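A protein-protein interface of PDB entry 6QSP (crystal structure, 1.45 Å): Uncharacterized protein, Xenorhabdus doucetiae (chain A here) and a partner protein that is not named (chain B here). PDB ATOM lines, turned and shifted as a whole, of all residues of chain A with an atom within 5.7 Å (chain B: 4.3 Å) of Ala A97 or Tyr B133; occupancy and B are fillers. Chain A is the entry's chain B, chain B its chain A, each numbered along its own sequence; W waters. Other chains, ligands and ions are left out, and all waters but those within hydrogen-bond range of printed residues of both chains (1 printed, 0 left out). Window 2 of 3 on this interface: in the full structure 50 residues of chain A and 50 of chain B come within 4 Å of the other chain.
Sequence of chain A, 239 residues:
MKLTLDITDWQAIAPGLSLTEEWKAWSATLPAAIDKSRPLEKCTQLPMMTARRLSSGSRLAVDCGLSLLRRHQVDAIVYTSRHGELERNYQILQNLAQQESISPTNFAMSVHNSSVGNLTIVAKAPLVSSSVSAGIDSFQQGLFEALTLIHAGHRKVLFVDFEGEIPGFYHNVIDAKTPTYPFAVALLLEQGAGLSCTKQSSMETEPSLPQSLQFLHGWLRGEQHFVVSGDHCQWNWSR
OH of Tyr B133 sits at hydrogen-bond distance from O of Ala A97, at 2.9 Å.
Among the printed residues, pairs that only touch across the chains: Gln A94 with Val B132, Ala A97 with Ser B129 and Gln A98 with Tyr B133.
Ala A97 touches just these residues of chain B: Ser B129 and Tyr B133.
Tyr B133 touches two residues of chain A.
Printed residues of chain B within 4 Å of Gln A94: Val B132 (3.5 Å).
Of the printed residues of chain A, Val B132 touches Gln A94 (3.5 Å).
Asn A95 touches none of the printed residues of chain B.
Ile A92 touches none of the printed residues of chain B.
The nearest printed residue of chain B that does not touch Ala A97 is Val B132 (4.8 Å).
Hydrophobic or aromatic side chains of chain A that line the printed part of chain B: Ala A97.
Among the printed residues, 4 pairs touch across the chains.
Among the printed residues, no Asp or Glu carboxylate lies within 4 Å of a Lys or Arg side-chain nitrogen of the other chain.
Water W1 lies within hydrogen-bond range of OG of Ser B129 and O of Leu A93.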
ATOM      1  N   ILE A  92      14.097 -12.519  13.007  1.00  0.00           N
ATOM      2  CA  ILE A  92      13.015 -13.138  13.821  1.00  0.00           C
ATOM      3  C   ILE A  92      11.659 -12.606  13.342  1.00  0.00           C
ATOM      4  O   ILE A  92      10.702 -13.407  13.280  1.00  0.00           O
ATOM      5  CB  ILE A  92      13.279 -12.949  15.325  1.00  0.00           C
ATOM      6  CG1 ILE A  92      14.542 -13.722  15.718  1.00  0.00           C
ATOM      7  CG2 ILE A  92      12.063 -13.379  16.136  1.00  0.00           C
ATOM      8  CD1 ILE A  92      15.090 -13.371  17.070  1.00  0.00           C
ATOM      9  N   LEU A  93      11.561 -11.325  12.996  1.00  0.00           N
ATOM     10  CA  LEU A  93      10.283 -10.777  12.482  1.00  0.00           C
ATOM     11  C   LEU A  93       9.973 -11.447  11.137  1.00  0.00           C
ATOM     12  O   LEU A  93       8.787 -11.718  10.872  1.00  0.00           O
ATOM     13  CB  LEU A  93      10.381  -9.252  12.397  1.00  0.00           C
ATOM     14  CG  LEU A  93      10.547  -8.523  13.730  1.00  0.00           C
ATOM     15  CD1 LEU A  93      10.575  -7.026  13.483  1.00  0.00           C
ATOM     16  CD2 LEU A  93       9.456  -8.900  14.725  1.00  0.00           C
ATOM     17  N   GLN A  94      10.993 -11.759  10.336  1.00  0.00           N
ATOM     18  CA  GLN A  94      10.799 -12.506   9.067  1.00  0.00           C
ATOM     19  C   GLN A  94      10.372 -13.946   9.389  1.00  0.00           C
ATOM     20  O   GLN A  94       9.467 -14.450   8.698  1.00  0.00           O
ATOM     21  CB  GLN A  94      12.061 -12.449   8.203  1.00  0.00           C
ATOM     22  CG  GLN A  94      12.172 -11.172   7.369  1.00  0.00           C
ATOM     23  CD  GLN A  94      11.218 -11.138   6.197  1.00  0.00           C
ATOM     24  OE1 GLN A  94      10.312 -11.958   6.084  1.00  0.00           O
ATOM     25  NE2 GLN A  94      11.413 -10.174   5.312  1.00  0.00           N
ATOM     26  N   ASN A  95      10.952 -14.594  10.407  1.00  0.00           N
ATOM     27  CA  ASN A  95      10.501 -15.958  10.810  1.00  0.00           C
ATOM     28  C   ASN A  95       8.991 -15.898  11.115  1.00  0.00           C
ATOM     29  O   ASN A  95       8.246 -16.795  10.679  1.00  0.00           O
ATOM     30  CB  ASN A  95      11.205 -16.518  12.054  1.00  0.00           C
ATOM     31  CG  ASN A  95      12.699 -16.725  11.938  1.00  0.00           C
ATOM     32  OD1 ASN A  95      13.406 -16.586  12.943  1.00  0.00           O
ATOM     33  ND2 ASN A  95      13.189 -17.084  10.755  1.00  0.00           N
ATOM     34  N   LEU A  96       8.553 -14.883  11.873  1.00  0.00           N
ATOM     35  CA  LEU A  96       7.123 -14.734  12.260  1.00  0.00           C
ATOM     36  C   LEU A  96       6.274 -14.497  11.001  1.00  0.00           C
ATOM     37  O   LEU A  96       5.213 -15.122  10.891  1.00  0.00           O
ATOM     38  CB  LEU A  96       6.953 -13.597  13.272  1.00  0.00           C
ATOM     39  CG  LEU A  96       7.557 -13.858  14.651  1.00  0.00           C
ATOM     40  CD1 LEU A  96       7.634 -12.570  15.441  1.00  0.00           C
ATOM     41  CD2 LEU A  96       6.762 -14.903  15.424  1.00  0.00           C
ATOM     42  N   ALA A  97       6.712 -13.641  10.074  1.00  0.00           N
ATOM     43  CA  ALA A  97       5.948 -13.331   8.839  1.00  0.00           C
ATOM     44  C   ALA A  97       5.810 -14.606   7.995  1.00  0.00           C
ATOM     45  O   ALA A  97       4.731 -14.833   7.406  1.00  0.00           O
ATOM     46  CB  ALA A  97       6.613 -12.219   8.066  1.00  0.00           C
ATOM     47  N   GLN A  98       6.861 -15.425   7.945  1.00  0.00           N
ATOM     48  CA  GLN A  98       6.914 -16.610   7.044  1.00  0.00           C
ATOM     49  C   GLN A  98       6.425 -17.871   7.768  1.00  0.00           C
ATOM     50  O   GLN A  98       6.437 -18.933   7.134  1.00  0.00           O
ATOM     51  CB  GLN A  98       8.339 -16.808   6.532  1.00  0.00           C
ATOM     52  CG  GLN A  98       8.848 -15.627   5.726  1.00  0.00           C
ATOM     53  CD  GLN A  98      10.210 -15.893   5.143  1.00  0.00           C
ATOM     54  OE1 GLN A  98      11.219 -15.364   5.605  1.00  0.00           O
ATOM     55  NE2 GLN A  98      10.244 -16.726   4.115  1.00  0.00           N
ATOM     56  N   GLN A  99       6.015 -17.754   9.036  1.00  0.00           N
ATOM     57  CA  GLN A  99       5.553 -18.884   9.885  1.00  0.00           C
ATOM     58  C   GLN A  99       6.644 -19.963   9.936  1.00  0.00           C
ATOM     59  O   GLN A  99       6.318 -21.168   9.787  1.00  0.00           O
ATOM     60  CB  GLN A  99       4.214 -19.403   9.362  1.00  0.00           C
ATOM     61  CG  GLN A  99       3.147 -18.323   9.295  1.00  0.00           C
ATOM     62  CD  GLN A  99       1.825 -18.872   8.832  1.00  0.00           C
ATOM     63  OE1 GLN A  99       1.212 -19.704   9.497  1.00  0.00           O
ATOM     64  NE2 GLN A  99       1.371 -18.403   7.682  1.00  0.00           N
ATOM     65  N   SER B 129       5.536  -7.727   8.514  1.00  0.00           N
ATOM     66  CA  SER B 129       4.461  -8.582   7.943  1.00  0.00           C
ATOM     67  C   SER B 129       3.653  -7.788   6.906  1.00  0.00           C
ATOM     68  O   SER B 129       3.362  -8.346   5.824  1.00  0.00           O
ATOM     69  CB  SER B 129       3.579  -9.160   9.014  1.00  0.00           C
ATOM     70  OG  SER B 129       4.222 -10.249   9.656  1.00  0.00           O
ATOM     71  N   ARG B 130       3.301  -6.537   7.204  1.00  0.00           N
ATOM     72  CA  ARG B 130       2.448  -5.723   6.297  1.00  0.00           C
ATOM     73  C   ARG B 130       3.245  -5.463   5.018  1.00  0.00           C
ATOM     74  O   ARG B 130       2.636  -5.429   3.930  1.00  0.00           O
ATOM     75  CB  ARG B 130       1.974  -4.421   6.963  1.00  0.00           C
ATOM     76  CG  ARG B 130       1.445  -3.366   6.001  1.00  0.00           C
ATOM     77  CD  ARG B 130       1.074  -2.049   6.670  1.00  0.00           C
ATOM     78  NE  ARG B 130       2.164  -1.435   7.430  1.00  0.00           N
ATOM     79  CZ  ARG B 130       3.191  -0.745   6.918  1.00  0.00           C
ATOM     80  NH1 ARG B 130       3.299  -0.562   5.610  1.00  0.00           N
ATOM     81  NH2 ARG B 130       4.110  -0.240   7.728  1.00  0.00           N
ATOM     82  N   THR B 131       4.550  -5.233   5.128  1.00  0.00           N
ATOM     83  CA  THR B 131       5.413  -4.923   3.959  1.00  0.00           C
ATOM     84  C   THR B 131       5.576  -6.195   3.119  1.00  0.00           C
ATOM     85  O   THR B 131       5.380  -6.118   1.879  1.00  0.00           O
ATOM     86  CB  THR B 131       6.767  -4.327   4.377  1.00  0.00           C
ATOM     87  OG1 THR B 131       6.520  -3.111   5.081  1.00  0.00           O
ATOM     88  CG2 THR B 131       7.677  -4.058   3.194  1.00  0.00           C
ATOM     89  N   VAL B 132       5.921  -7.321   3.755  1.00  0.00           N
ATOM     90  CA  VAL B 132       6.245  -8.598   3.048  1.00  0.00           C
ATOM     91  C   VAL B 132       5.021  -9.039   2.246  1.00  0.00           C
ATOM     92  O   VAL B 132       5.189  -9.433   1.069  1.00  0.00           O
ATOM     93  CB  VAL B 132       6.724  -9.693   4.027  1.00  0.00           C
ATOM     94  CG1 VAL B 132       6.642 -11.095   3.419  1.00  0.00           C
ATOM     95  CG2 VAL B 132       8.131  -9.386   4.512  1.00  0.00           C
ATOM     96  N   TYR B 133       3.820  -8.919   2.813  1.00  0.00           N
ATOM     97  CA  TYR B 133       2.593  -9.448   2.161  1.00  0.00           C
ATOM     98  C   TYR B 133       1.703  -8.335   1.604  1.00  0.00           C
ATOM     99  O   TYR B 133       0.636  -8.683   1.075  1.00  0.00           O
ATOM    100  CB  TYR B 133       1.850 -10.362   3.130  1.00  0.00           C
ATOM    101  CG  TYR B 133       2.643 -11.589   3.485  1.00  0.00           C
ATOM    102  CD1 TYR B 133       3.073 -12.471   2.505  1.00  0.00           C
ATOM    103  CD2 TYR B 133       2.969 -11.865   4.799  1.00  0.00           C
ATOM    104  CE1 TYR B 133       3.809 -13.603   2.823  1.00  0.00           C
ATOM    105  CE2 TYR B 133       3.703 -12.987   5.135  1.00  0.00           C
ATOM    106  CZ  TYR B 133       4.129 -13.855   4.147  1.00  0.00           C
ATOM    107  OH  TYR B 133       4.839 -14.966   4.484  1.00  0.00           O
ATOM    108  N   GLN B 134       2.154  -7.079   1.641  1.00  0.00           N
ATOM    109  CA  GLN B 134       1.433  -5.922   1.041  1.00  0.00           C
ATOM    110  C   GLN B 134       0.017  -5.880   1.630  1.00  0.00           C
ATOM    111  O   GLN B 134      -0.967  -5.746   0.885  1.00  0.00           O
ATOM    112  CB  GLN B 134       1.448  -6.014  -0.485  1.00  0.00           C
ATOM    113  CG  GLN B 134       2.855  -6.045  -1.058  1.00  0.00           C
ATOM    114  CD  GLN B 134       2.873  -5.936  -2.559  1.00  0.00           C
ATOM    115  OE1 GLN B 134       2.022  -6.494  -3.245  1.00  0.00           O
ATOM    116  NE2 GLN B 134       3.859  -5.227  -3.079  1.00  0.00           N
ATOM    117  N   GLN B 135      -0.071  -6.003   2.948  1.00  0.00           N
ATOM    118  CA  GLN B 135      -1.351  -6.029   3.694  1.00  0.00           C
ATOM    119  C   GLN B 135      -1.852  -4.587   3.822  1.00  0.00           C
ATOM    120  O   GLN B 135      -1.051  -3.699   4.142  1.00  0.00           O
ATOM    121  CB  GLN B 135      -1.155  -6.696   5.054  1.00  0.00           C
ATOM    122  CG  GLN B 135      -0.566  -8.096   4.958  1.00  0.00           C
ATOM    123  CD  GLN B 135      -0.251  -8.701   6.301  1.00  0.00           C
ATOM    124  OE1 GLN B 135      -0.021  -7.995   7.278  1.00  0.00           O
ATOM    125  NE2 GLN B 135      -0.234 -10.026   6.355  1.00  0.00           N
HETATM  126  O   HOH W   1       6.669  -9.855  10.884  1.00  0.00           O
